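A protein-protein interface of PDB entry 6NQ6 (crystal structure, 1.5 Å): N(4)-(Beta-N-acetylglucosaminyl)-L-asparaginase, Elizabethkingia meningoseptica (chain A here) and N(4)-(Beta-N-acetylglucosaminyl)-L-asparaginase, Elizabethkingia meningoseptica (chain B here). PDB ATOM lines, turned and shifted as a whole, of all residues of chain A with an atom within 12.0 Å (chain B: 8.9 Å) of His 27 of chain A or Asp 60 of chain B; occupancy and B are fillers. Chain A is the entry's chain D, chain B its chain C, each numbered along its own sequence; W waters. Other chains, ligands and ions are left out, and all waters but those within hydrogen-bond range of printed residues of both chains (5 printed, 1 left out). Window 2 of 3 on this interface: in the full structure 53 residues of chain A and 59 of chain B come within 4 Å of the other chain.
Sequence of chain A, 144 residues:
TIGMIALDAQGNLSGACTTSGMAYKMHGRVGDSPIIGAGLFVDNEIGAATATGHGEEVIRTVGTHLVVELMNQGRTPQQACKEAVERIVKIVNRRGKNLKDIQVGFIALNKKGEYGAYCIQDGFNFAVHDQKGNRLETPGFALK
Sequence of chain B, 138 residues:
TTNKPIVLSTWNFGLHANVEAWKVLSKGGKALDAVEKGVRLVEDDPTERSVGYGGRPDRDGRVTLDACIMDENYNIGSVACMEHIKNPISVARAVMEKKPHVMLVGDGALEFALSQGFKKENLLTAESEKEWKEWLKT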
ATOM      1  N   SER A  20      -2.367  -8.708  22.172  1.00  0.00           N
ATOM      2  CA  SER A  20      -1.311  -7.720  22.134  1.00  0.00           C
ATOM      3  C   SER A  20      -1.591  -6.647  21.103  1.00  0.00           C
ATOM      4  O   SER A  20      -0.750  -5.731  20.942  1.00  0.00           O
ATOM      5  CB  SER A  20       0.045  -8.397  21.938  1.00  0.00           C
ATOM      6  OG  SER A  20       0.116  -9.152  20.791  1.00  0.00           O
ATOM      7  N   GLY A  21      -2.661  -6.756  20.312  1.00  0.00           N
ATOM      8  CA  GLY A  21      -2.994  -5.696  19.353  1.00  0.00           C
ATOM      9  C   GLY A  21      -2.116  -5.706  18.110  1.00  0.00           C
ATOM     10  O   GLY A  21      -1.342  -6.649  17.879  1.00  0.00           O
ATOM     11  N   MET A  22      -2.273  -4.663  17.294  1.00  0.00           N
ATOM     12  CA  MET A  22      -1.640  -4.624  15.936  1.00  0.00           C
ATOM     13  C   MET A  22      -0.154  -4.449  16.123  1.00  0.00           C
ATOM     14  O   MET A  22       0.274  -3.586  16.897  1.00  0.00           O
ATOM     15  CB  MET A  22      -2.198  -3.470  15.122  1.00  0.00           C
ATOM     16  CG  MET A  22      -1.682  -3.512  13.691  1.00  0.00           C
ATOM     17  SD  MET A  22      -2.152  -2.023  12.807  1.00  0.00           S
ATOM     18  CE  MET A  22      -0.601  -1.095  12.775  1.00  0.00           C
ATOM     19  N   ALA A  23       0.651  -5.282  15.460  1.00  0.00           N
ATOM     20  CA  ALA A  23       2.085  -5.105  15.588  1.00  0.00           C
ATOM     21  C   ALA A  23       2.497  -3.737  15.068  1.00  0.00           C
ATOM     22  O   ALA A  23       2.017  -3.297  14.011  1.00  0.00           O
ATOM     23  CB  ALA A  23       2.880  -6.172  14.839  1.00  0.00           C
ATOM     24  N   TYR A  24       3.284  -3.082  15.906  1.00  0.00           N
ATOM     25  CA  TYR A  24       3.979  -1.836  15.581  1.00  0.00           C
ATOM     26  C   TYR A  24       2.997  -0.656  15.415  1.00  0.00           C
ATOM     27  O   TYR A  24       3.219   0.317  14.747  1.00  0.00           O
ATOM     28  CB  TYR A  24       4.903  -2.014  14.349  1.00  0.00           C
ATOM     29  CG  TYR A  24       5.685  -3.309  14.382  1.00  0.00           C
ATOM     30  CD1 TYR A  24       6.373  -3.703  15.530  1.00  0.00           C
ATOM     31  CD2 TYR A  24       5.705  -4.134  13.258  1.00  0.00           C
ATOM     32  CE1 TYR A  24       7.086  -4.898  15.555  1.00  0.00           C
ATOM     33  CE2 TYR A  24       6.419  -5.339  13.272  1.00  0.00           C
ATOM     34  CZ  TYR A  24       7.079  -5.699  14.427  1.00  0.00           C
ATOM     35  OH  TYR A  24       7.802  -6.866  14.531  1.00  0.00           O
ATOM     36  N   LYS A  25       1.846  -0.814  16.052  1.00  0.00           N
ATOM     37  CA  LYS A  25       0.871   0.219  16.223  1.00  0.00           C
ATOM     38  C   LYS A  25       1.435   1.489  16.829  1.00  0.00           C
ATOM     39  O   LYS A  25       2.359   1.457  17.621  1.00  0.00           O
ATOM     40  CB  LYS A  25      -0.300  -0.329  17.097  1.00  0.00           C
ATOM     41  CG  LYS A  25       0.059  -0.600  18.537  1.00  0.00           C
ATOM     42  CD  LYS A  25      -0.861  -1.630  19.267  1.00  0.00           C
ATOM     43  CE  LYS A  25      -0.454  -1.831  20.722  1.00  0.00           C
ATOM     44  NZ  LYS A  25      -1.054  -2.992  21.476  1.00  0.00           N
ATOM     45  N   MET A  26       0.723   2.588  16.641  1.00  0.00           N
ATOM     46  CA  MET A  26       1.080   3.811  17.329  1.00  0.00           C
ATOM     47  C   MET A  26       0.878   3.617  18.845  1.00  0.00           C
ATOM     48  O   MET A  26      -0.010   2.917  19.262  1.00  0.00           O
ATOM     49  CB  MET A  26       0.169   4.931  16.822  1.00  0.00           C
ATOM     50  CG  MET A  26       0.349   6.283  17.473  1.00  0.00           C
ATOM     51  SD  MET A  26      -0.734   7.542  16.720  1.00  0.00           S
ATOM     52  CE  MET A  26      -1.826   6.400  15.761  1.00  0.00           C
ATOM     53  N   HIS A  27       1.718   4.213  19.673  1.00  0.00           N
ATOM     54  CA  HIS A  27       1.570   4.056  21.063  1.00  0.00           C
ATOM     55  C   HIS A  27       0.132   4.502  21.478  1.00  0.00           C
ATOM     56  O   HIS A  27      -0.356   5.557  21.036  1.00  0.00           O
ATOM     57  CB  HIS A  27       2.588   4.899  21.851  1.00  0.00           C
ATOM     58  CG  HIS A  27       2.564   4.619  23.314  1.00  0.00           C
ATOM     59  ND1 HIS A  27       2.824   3.362  23.830  1.00  0.00           N
ATOM     60  CD2 HIS A  27       2.300   5.414  24.380  1.00  0.00           C
ATOM     61  CE1 HIS A  27       2.695   3.393  25.144  1.00  0.00           C
ATOM     62  NE2 HIS A  27       2.368   4.624  25.508  1.00  0.00           N
ATOM     63  N   GLY A  28      -0.527   3.693  22.320  1.00  0.00           N
ATOM     64  CA  GLY A  28      -1.813   3.990  22.861  1.00  0.00           C
ATOM     65  C   GLY A  28      -2.957   3.473  21.976  1.00  0.00           C
ATOM     66  O   GLY A  28      -4.122   3.637  22.395  1.00  0.00           O
ATOM     67  N   ARG A  29      -2.665   2.789  20.885  1.00  0.00           N
ATOM     68  CA  ARG A  29      -3.656   2.184  19.983  1.00  0.00           C
ATOM     69  C   ARG A  29      -4.447   1.059  20.713  1.00  0.00           C
ATOM     70  O   ARG A  29      -3.833   0.167  21.242  1.00  0.00           O
ATOM     71  CB  ARG A  29      -3.192   1.789  18.701  1.00  0.00           C
ATOM     72  CG  ARG A  29      -4.278   1.231  17.746  1.00  0.00           C
ATOM     73  CD  ARG A  29      -4.528  -0.253  18.012  1.00  0.00           C
ATOM     74  NE  ARG A  29      -5.471  -1.008  17.163  1.00  0.00           N
ATOM     75  CZ  ARG A  29      -5.510  -2.333  17.160  1.00  0.00           C
ATOM     76  NH1 ARG A  29      -4.563  -2.939  17.919  1.00  0.00           N
ATOM     77  NH2 ARG A  29      -6.397  -2.988  16.392  1.00  0.00           N
ATOM     78  N   VAL A  30      -5.785   1.142  20.749  1.00  0.00           N
ATOM     79  CA  VAL A  30      -6.629   0.093  21.308  1.00  0.00           C
ATOM     80  C   VAL A  30      -7.616  -0.296  20.212  1.00  0.00           C
ATOM     81  O   VAL A  30      -8.204   0.575  19.566  1.00  0.00           O
ATOM     82  CB  VAL A  30      -7.387   0.631  22.546  1.00  0.00           C
ATOM     83  CG1 VAL A  30      -8.347  -0.430  23.077  1.00  0.00           C
ATOM     84  CG2 VAL A  30      -6.490   1.166  23.647  1.00  0.00           C
ATOM     85  N   GLY A  31      -7.778  -1.589  19.994  1.00  0.00           N
ATOM     86  CA  GLY A  31      -8.735  -2.164  19.167  1.00  0.00           C
ATOM     87  C   GLY A  31     -10.014  -2.618  19.825  1.00  0.00           C
ATOM     88  O   GLY A  31     -10.426  -2.090  20.843  1.00  0.00           O
ATOM     89  N   ARG B  56       3.968  -8.914  19.747  1.00  0.00           N
ATOM     90  CA  ARG B  56       4.713  -7.876  18.977  1.00  0.00           C
ATOM     91  C   ARG B  56       4.397  -6.492  19.557  1.00  0.00           C
ATOM     92  O   ARG B  56       3.228  -6.113  19.718  1.00  0.00           O
ATOM     93  CB  ARG B  56       4.432  -7.912  17.503  1.00  0.00           C
ATOM     94  CG  ARG B  56       4.772  -9.238  16.854  1.00  0.00           C
ATOM     95  CD  ARG B  56       4.747  -9.176  15.350  1.00  0.00           C
ATOM     96  NE  ARG B  56       5.012 -10.527  14.830  1.00  0.00           N
ATOM     97  CZ  ARG B  56       4.079 -11.486  14.703  1.00  0.00           C
ATOM     98  NH1 ARG B  56       2.797 -11.291  15.029  1.00  0.00           N
ATOM     99  NH2 ARG B  56       4.423 -12.687  14.222  1.00  0.00           N
ATOM    100  N   PRO B  57       5.426  -5.725  19.894  1.00  0.00           N
ATOM    101  CA  PRO B  57       5.238  -4.447  20.493  1.00  0.00           C
ATOM    102  C   PRO B  57       4.679  -3.386  19.522  1.00  0.00           C
ATOM    103  O   PRO B  57       4.557  -3.610  18.281  1.00  0.00           O
ATOM    104  CB  PRO B  57       6.685  -4.060  20.925  1.00  0.00           C
ATOM    105  CG  PRO B  57       7.500  -4.620  19.822  1.00  0.00           C
ATOM    106  CD  PRO B  57       6.848  -5.973  19.568  1.00  0.00           C
ATOM    107  N   ASP B  58       4.300  -2.265  20.130  1.00  0.00           N
ATOM    108  CA  ASP B  58       3.964  -1.035  19.413  1.00  0.00           C
ATOM    109  C   ASP B  58       5.264  -0.484  18.774  1.00  0.00           C
ATOM    110  O   ASP B  58       6.342  -1.055  19.004  1.00  0.00           O
ATOM    111  CB  ASP B  58       3.200  -0.051  20.298  1.00  0.00           C
ATOM    112  CG  ASP B  58       4.047   0.691  21.318  1.00  0.00           C
ATOM    113  OD1 ASP B  58       5.344   0.727  21.174  1.00  0.00           O
ATOM    114  OD2 ASP B  58       3.476   1.303  22.227  1.00  0.00           O
ATOM    115  N   ARG B  59       5.135   0.562  17.994  1.00  0.00           N
ATOM    116  CA  ARG B  59       6.258   1.050  17.163  1.00  0.00           C
ATOM    117  C   ARG B  59       7.362   1.594  17.967  1.00  0.00           C
ATOM    118  O   ARG B  59       8.511   1.663  17.426  1.00  0.00           O
ATOM    119  CB  ARG B  59       5.780   2.096  16.148  1.00  0.00           C
ATOM    120  CG  ARG B  59       5.239   3.385  16.754  1.00  0.00           C
ATOM    121  CD  ARG B  59       4.717   4.226  15.577  1.00  0.00           C
ATOM    122  NE  ARG B  59       4.356   5.555  16.010  1.00  0.00           N
ATOM    123  CZ  ARG B  59       3.888   6.509  15.200  1.00  0.00           C
ATOM    124  NH1 ARG B  59       3.606   6.272  13.933  1.00  0.00           N
ATOM    125  NH2 ARG B  59       3.630   7.719  15.697  1.00  0.00           N
ATOM    126  N   ASP B  60       7.099   1.948  19.208  1.00  0.00           N
ATOM    127  CA  ASP B  60       8.144   2.362  20.142  1.00  0.00           C
ATOM    128  C   ASP B  60       8.776   1.259  20.922  1.00  0.00           C
ATOM    129  O   ASP B  60       9.551   1.560  21.831  1.00  0.00           O
ATOM    130  CB  ASP B  60       7.630   3.473  21.044  1.00  0.00           C
ATOM    131  CG  ASP B  60       7.156   4.675  20.255  1.00  0.00           C
ATOM    132  OD1 ASP B  60       7.775   5.054  19.227  1.00  0.00           O
ATOM    133  OD2 ASP B  60       6.128   5.271  20.611  1.00  0.00           O
ATOM    134  N   GLY B  61       8.481  -0.010  20.596  1.00  0.00           N
ATOM    135  CA  GLY B  61       9.018  -1.142  21.388  1.00  0.00           C
ATOM    136  C   GLY B  61       8.314  -1.512  22.660  1.00  0.00           C
ATOM    137  O   GLY B  61       8.856  -2.262  23.453  1.00  0.00           O
ATOM    138  N   ARG B  62       7.083  -0.995  22.879  1.00  0.00           N
ATOM    139  CA  ARG B  62       6.344  -1.205  24.138  1.00  0.00           C
ATOM    140  C   ARG B  62       5.308  -2.267  23.897  1.00  0.00           C
ATOM    141  O   ARG B  62       4.519  -2.137  22.965  1.00  0.00           O
ATOM    142  CB  ARG B  62       5.712   0.111  24.584  1.00  0.00           C
ATOM    143  CG  ARG B  62       6.797   1.096  24.957  1.00  0.00           C
ATOM    144  CD  ARG B  62       6.270   2.469  25.286  1.00  0.00           C
ATOM    145  NE  ARG B  62       5.565   2.562  26.584  1.00  0.00           N
ATOM    146  CZ  ARG B  62       5.225   3.726  27.156  1.00  0.00           C
ATOM    147  NH1 ARG B  62       5.504   4.906  26.552  1.00  0.00           N
ATOM    148  NH2 ARG B  62       4.572   3.732  28.311  1.00  0.00           N
ATOM    149  N   VAL B  63       5.390  -3.349  24.640  1.00  0.00           N
ATOM    150  CA  VAL B  63       4.295  -4.368  24.527  1.00  0.00           C
ATOM    151  C   VAL B  63       3.108  -3.882  25.396  1.00  0.00           C
ATOM    152  O   VAL B  63       3.172  -3.812  26.634  1.00  0.00           O
ATOM    153  CB  VAL B  63       4.760  -5.715  25.043  1.00  0.00           C
ATOM    154  CG1 VAL B  63       3.545  -6.686  25.002  1.00  0.00           C
ATOM    155  CG2 VAL B  63       5.897  -6.293  24.181  1.00  0.00           C
ATOM    156  N   THR B  64       2.040  -3.484  24.716  1.00  0.00           N
ATOM    157  CA  THR B  64       0.838  -3.005  25.383  1.00  0.00           C
ATOM    158  C   THR B  64      -0.252  -4.032  25.150  1.00  0.00           C
ATOM    159  O   THR B  64      -0.468  -4.462  24.016  1.00  0.00           O
ATOM    160  CB  THR B  64       0.384  -1.643  24.832  1.00  0.00           C
ATOM    161  OG1 THR B  64       0.206  -1.733  23.414  1.00  0.00           O
ATOM    162  CG2 THR B  64       1.421  -0.572  25.141  1.00  0.00           C
ATOM    163  N   LEU B  65      -0.943  -4.434  26.209  1.00  0.00           N
ATOM    164  CA  LEU B  65      -1.999  -5.465  26.041  1.00  0.00           C
ATOM    165  C   LEU B  65      -3.387  -4.948  26.395  1.00  0.00           C
ATOM    166  O   LEU B  65      -3.528  -4.080  27.238  1.00  0.00           O
ATOM    167  CB  LEU B  65      -1.636  -6.596  26.974  1.00  0.00           C
ATOM    168  CG  LEU B  65      -0.226  -7.215  26.845  1.00  0.00           C
ATOM    169  CD1 LEU B  65      -0.160  -8.392  27.822  1.00  0.00           C
ATOM    170  CD2 LEU B  65       0.057  -7.655  25.433  1.00  0.00           C
ATOM    171  N   CYS B  81      -4.197  -1.118  26.829  1.00  0.00           N
ATOM    172  CA  CYS B  81      -2.880  -0.501  26.738  1.00  0.00           C
ATOM    173  C   CYS B  81      -2.115  -0.630  28.034  1.00  0.00           C
ATOM    174  O   CYS B  81      -1.655   0.363  28.610  1.00  0.00           O
ATOM    175  CB  CYS B  81      -3.005   0.948  26.285  1.00  0.00           C
ATOM    176  SG  CYS B  81      -1.403   1.641  25.680  1.00  0.00           S
ATOM    177  N   MET B  82      -2.095  -1.861  28.557  1.00  0.00           N
ATOM    178  CA  MET B  82      -1.466  -2.148  29.839  1.00  0.00           C
ATOM    179  C   MET B  82      -0.100  -2.813  29.561  1.00  0.00           C
ATOM    180  O   MET B  82       0.019  -3.711  28.739  1.00  0.00           O
ATOM    181  CB  MET B  82      -2.306  -3.037  30.753  1.00  0.00           C
ATOM    182  CG  MET B  82      -1.718  -3.193  32.122  1.00  0.00           C
ATOM    183  SD  MET B  82      -2.756  -4.199  33.213  1.00  0.00           S
ATOM    184  CE  MET B  82      -2.902  -5.721  32.254  1.00  0.00           C
ATOM    185  N   GLU B  83       0.931  -2.377  30.292  1.00  0.00           N
ATOM    186  CA  GLU B  83       2.295  -2.931  30.131  1.00  0.00           C
ATOM    187  C   GLU B  83       2.686  -3.737  31.342  1.00  0.00           C
ATOM    188  O   GLU B  83       2.196  -3.513  32.444  1.00  0.00           O
ATOM    189  CB  GLU B  83       3.334  -1.808  30.060  1.00  0.00           C
ATOM    190  CG  GLU B  83       3.213  -0.976  28.812  1.00  0.00           C
ATOM    191  CD  GLU B  83       4.075   0.283  28.866  1.00  0.00           C
ATOM    192  OE1 GLU B  83       3.540   1.344  29.296  1.00  0.00           O
ATOM    193  OE2 GLU B  83       5.245   0.202  28.433  1.00  0.00           O
ATOM    194  N   GLY B 106      -3.847   2.163  30.315  1.00  0.00           N
ATOM    195  CA  GLY B 106      -2.530   2.815  30.426  1.00  0.00           C
ATOM    196  C   GLY B 106      -1.909   2.649  31.824  1.00  0.00           C
ATOM    197  O   GLY B 106      -1.987   1.576  32.467  1.00  0.00           O
ATOM    198  N   ASP B 107      -1.218   3.674  32.316  1.00  0.00           N
ATOM    199  CA  ASP B 107      -0.492   3.526  33.619  1.00  0.00           C
ATOM    200  C   ASP B 107      -1.395   3.094  34.787  1.00  0.00           C
ATOM    201  O   ASP B 107      -1.005   2.296  35.677  1.00  0.00           O
ATOM    202  CB  ASP B 107       0.176   4.844  34.058  1.00  0.00           C
ATOM    203  CG  ASP B 107       1.251   5.302  33.142  1.00  0.00           C
ATOM    204  OD1 ASP B 107       1.799   4.530  32.347  1.00  0.00           O
ATOM    205  OD2 ASP B 107       1.593   6.521  33.196  1.00  0.00           O
ATOM    206  N   LEU B 124       8.729  -8.303  26.485  1.00  0.00           N
ATOM    207  CA  LEU B 124       9.370  -8.274  25.190  1.00  0.00           C
ATOM    208  C   LEU B 124      10.411  -9.416  25.093  1.00  0.00           C
ATOM    209  O   LEU B 124      11.432  -9.408  25.808  1.00  0.00           O
ATOM    210  CB  LEU B 124      10.013  -6.899  24.988  1.00  0.00           C
ATOM    211  CG  LEU B 124      10.585  -6.604  23.610  1.00  0.00           C
ATOM    212  CD1 LEU B 124       9.492  -6.605  22.535  1.00  0.00           C
ATOM    213  CD2 LEU B 124      11.343  -5.271  23.628  1.00  0.00           C
ATOM    214  N   TRP B 132      11.184  -6.260  15.831  1.00  0.00           N
ATOM    215  CA  TRP B 132      10.743  -4.861  15.960  1.00  0.00           C
ATOM    216  C   TRP B 132      11.865  -3.930  15.462  1.00  0.00           C
ATOM    217  O   TRP B 132      11.610  -3.044  14.612  1.00  0.00           O
ATOM    218  CB  TRP B 132      10.369  -4.506  17.415  1.00  0.00           C
ATOM    219  CG  TRP B 132      10.406  -3.017  17.669  1.00  0.00           C
ATOM    220  CD1 TRP B 132       9.588  -2.092  17.089  1.00  0.00           C
ATOM    221  CD2 TRP B 132      11.195  -2.301  18.638  1.00  0.00           C
ATOM    222  NE1 TRP B 132       9.857  -0.871  17.568  1.00  0.00           N
ATOM    223  CE2 TRP B 132      10.864  -0.928  18.483  1.00  0.00           C
ATOM    224  CE3 TRP B 132      12.230  -2.651  19.507  1.00  0.00           C
ATOM    225  CZ2 TRP B 132      11.463   0.091  19.239  1.00  0.00           C
ATOM    226  CZ3 TRP B 132      12.827  -1.632  20.278  1.00  0.00           C
ATOM    227  CH2 TRP B 132      12.442  -0.266  20.125  1.00  0.00           C
ATOM    228  N   LYS B 133      13.091  -4.153  15.949  1.00  0.00           N
ATOM    229  CA  LYS B 133      14.274  -3.482  15.404  1.00  0.00           C
ATOM    230  C   LYS B 133      14.462  -3.687  13.899  1.00  0.00           C
ATOM    231  O   LYS B 133      14.792  -2.727  13.209  1.00  0.00           O
ATOM    232  CB  LYS B 133      15.530  -3.869  16.213  1.00  0.00           C
ATOM    233  CG  LYS B 133      15.568  -3.176  17.565  1.00  0.00           C
ATOM    234  CD  LYS B 133      16.849  -3.420  18.357  1.00  0.00           C
ATOM    235  CE  LYS B 133      16.844  -2.554  19.603  1.00  0.00           C
ATOM    236  NZ  LYS B 133      17.827  -2.993  20.630  1.00  0.00           N
ATOM    237  N   TRP B 135      11.962  -4.082  11.860  1.00  0.00           N
ATOM    238  CA  TRP B 135      10.830  -3.409  11.270  1.00  0.00           C
ATOM    239  C   TRP B 135      11.147  -1.940  11.146  1.00  0.00           C
ATOM    240  O   TRP B 135      10.779  -1.296  10.164  1.00  0.00           O
ATOM    241  CB  TRP B 135       9.567  -3.617  12.130  1.00  0.00           C
ATOM    242  CG  TRP B 135       8.440  -2.721  11.676  1.00  0.00           C
ATOM    243  CD1 TRP B 135       7.614  -2.962  10.649  1.00  0.00           C
ATOM    244  CD2 TRP B 135       8.041  -1.468  12.233  1.00  0.00           C
ATOM    245  NE1 TRP B 135       6.717  -1.933  10.506  1.00  0.00           N
ATOM    246  CE2 TRP B 135       6.962  -1.001  11.467  1.00  0.00           C
ATOM    247  CE3 TRP B 135       8.478  -0.698  13.319  1.00  0.00           C
ATOM    248  CZ2 TRP B 135       6.310   0.217  11.735  1.00  0.00           C
ATOM    249  CZ3 TRP B 135       7.823   0.535  13.582  1.00  0.00           C
ATOM    250  CH2 TRP B 135       6.767   0.968  12.780  1.00  0.00           C
ATOM    251  N   LEU B 136      11.824  -1.419  12.161  1.00  0.00           N
ATOM    252  CA  LEU B 136      12.286  -0.023  12.164  1.00  0.00           C
ATOM    253  C   LEU B 136      13.183   0.306  10.971  1.00  0.00           C
ATOM    254  O   LEU B 136      13.136   1.429  10.451  1.00  0.00           O
ATOM    255  CB  LEU B 136      13.032   0.323  13.464  1.00  0.00           C
ATOM    256  CG  LEU B 136      12.275   0.511  14.779  1.00  0.00           C
ATOM    257  CD1 LEU B 136      13.242   0.552  15.964  1.00  0.00           C
ATOM    258  CD2 LEU B 136      11.439   1.774  14.804  1.00  0.00           C
HETATM  259  O   HOH W   1       1.108  -7.535  18.827  1.00  0.00           O
HETATM  260  O   HOH W   2       0.809   1.123  22.614  1.00  0.00           O
HETATM  261  O   HOH W   3       1.762  -4.725  21.968  1.00  0.00           O
HETATM  262  O   HOH W   4      -2.689  -1.265  23.519  1.00  0.00           O
HETATM  263  O   HOH W   5       4.097   5.907  18.954  1.00  0.00           O
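The backbone carbonyl oxygen of Pro 57 of chain B sits at hydrogen-bond distance from the backbone NH of Tyr 24 of chain A, 2.7 Å away. The side-chain carboxylate of Asp 58 of chain B lies within hydrogen-bond range of a ring nitrogen (ND1) of His 27 of chain A, at 2.7 Å. The backbone carbonyl oxygen of Lys 25 of chain A lies within hydrogen-bond range of the backbone NH of Arg 59 of chain B (2.9 Å). A ring nitrogen (NE2) of His 27 of chain A is in hydrogen-bond range of the guanidinium group (NH1) of Arg 62 of chain B (3.3 Å). The side-chain amino group (NZ) of Lys 25 of chain A is in hydrogen-bond range of the side-chain hydroxyl (OG1) of Thr 64 of chain B. The backbone carbonyl oxygen of Ser 20 of chain A lies close to the backbone carbonyl oxygen of Thr 64 of chain B (3.3 Å).
The side-chain carboxylate (OD1) of Asp 58 of chain B sits at hydrogen-bond distance from the backbone NH (N) of Arg 62 of chain B, 3.0 Å away. The guanidinium group (NH2) of Arg 62 of chain B lies within salt-bridge range of the side-chain carboxylate (OE1) of Glu 83 of chain B, at 2.8 Å. The backbone carbonyl oxygen (O) of Leu 65 of chain B sits at hydrogen-bond distance from the backbone NH (N) of Cys 81 of chain B (3.1 Å). The backbone NH (N) of Leu 65 of chain B sits at hydrogen-bond distance from the backbone carbonyl oxygen (O) of Met 82 of chain B, 2.8 Å away. O of Cys 81 of chain B sits close to N of Gly 106 of chain B, 3.3 Å away. O of Ser 20 of chain A lies within hydrogen-bond range of NZ of Lys 25 of chain A (2.8 Å).
Among the printed residues, merely in contact across the chains: Lys 25 of chain A with Asp 58 of chain B, Tyr 24 of chain A with Arg 59 of chain B, Tyr 24 of chain A with Trp 135 of chain B, Ala 23 of chain A with Arg 56 of chain B, Ser 20 of chain A with Leu 65 of chain B, Tyr 24 of chain A with Trp 132 of chain B, Gly 28 of chain A with Cys 81 of chain B, Tyr 24 of chain A with Asp 58 of chain B, His 27 of chain A with Asp 60 of chain B, Ala 23 of chain A with Pro 57 of chain B, Tyr 24 of chain A with Arg 56 of chain B, Met 26 of chain A with Arg 59 of chain B and Ser 20 of chain A with Arg 56 of chain B.
Printed residues of chain B within 4 Å of His 27 of chain A: Asp 58 (2.7 Å), Asp 60 (3.8 Å) and Arg 62 (3.2 Å). Of chain B, only Cys 81 (3.7 Å) comes within 4 Å of Gly 28 of chain A. Pro 57 of chain B touches just these residues of chain A: Ala 23 and Tyr 24. Of chain A, only Tyr 24 (3.7 Å), Lys 25 (3.2 Å) and His 27 (2.7 Å) come within 4 Å of Asp 58 of chain B. Of chain A, only Tyr 24, Lys 25 and Met 26 come within 4 Å of Arg 59 of chain B. No residue of chain A comes within 4 Å of Gly 61 of chain B. Arg 62 of chain B touches just one residue of chain A: His 27. Printed residues of chain A within 4 Å of Trp 135 of chain B: Tyr 24 (3.4 Å). Printed residues of chain B within 4 Å of Ser 20 of chain A: Arg 56, Thr 64 and Leu 65. Of the printed residues of chain A, Thr 64 of chain B touches Ser 20 and Lys 25. Of the printed residues of chain B, Tyr 24 of chain A touches Arg 56 (3.9 Å), Pro 57 (2.7 Å), Asp 58 (3.7 Å), Arg 59 (3.4 Å), Trp 132 (3.7 Å) and Trp 135 (3.4 Å). Of the printed residues of chain B, Met 26 of chain A touches Arg 59. Leu 124 of chain B touches none of the printed residues of chain A. The nearest residue of chain B that does not touch His 27 of chain A is Thr 64 of chain B (4.2 Å). The nearest printed residue of chain A that does not touch Cys 81 of chain B is Val 30 of chain A (4.4 Å).
Of the 12 printed residues of chain A, 7 touch a printed residue of chain B. Hydrophobic or aromatic side chains of chain A that line the printed part of chain B: Ala 23, Tyr 24, Met 26 and His 27. Of the 20 printed residues of chain B, 11 touch a printed residue of chain A. Hydrophobic or aromatic side chains of chain B within 4 Å of the printed part of chain A: Leu 65, Trp 132 and Trp 135. Along chain B the printed residues that touch a printed residue of chain A span positions 56 to 135. Among the printed residues, 19 pairs touch across the chains. Among the printed residues, no Asp or Glu carboxylate lies within 4 Å of a Lys or Arg side-chain nitrogen of the other chain.
Water W5 lies within hydrogen-bond range of OD2 of Asp 60 of chain B (2.7 Å), NE of Arg 59 of chain B (3.0 Å) and N of His 27 of chain A (3.0 Å). Water W2 lies within hydrogen-bond range of OD2 of Asp 58 of chain B (2.7 Å), N of Gly 28 of chain A (2.9 Å), OG1 of Thr 64 of chain B (3.0 Å) and ND1 of His 27 of chain A (3.2 Å). Water W1 lies within hydrogen-bond range of O of Arg 56 of chain B (2.7 Å), OG of Ser 20 of chain A (2.7 Å) and O of Gly 21 of chain A (2.8 Å). Water W3 lies within hydrogen-bond range of the backbone carbonyl oxygen of Ser 20 of chain A (2.9 Å), the backbone carbonyl oxygen of Arg 56 of chain B (3.0 Å), the backbone NH of Thr 64 of chain B (3.0 Å) and the side-chain amino group of Lys 25 of chain A (3.3 Å). Water W4 lies within hydrogen-bond range of the backbone carbonyl oxygen (O) of Arg 29 of chain A (2.9 Å), the side-chain hydroxyl (OG1) of Thr 64 of chain B (2.9 Å) and the side-chain amino group (NZ) of Lys 25 of chain A (3.1 Å).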
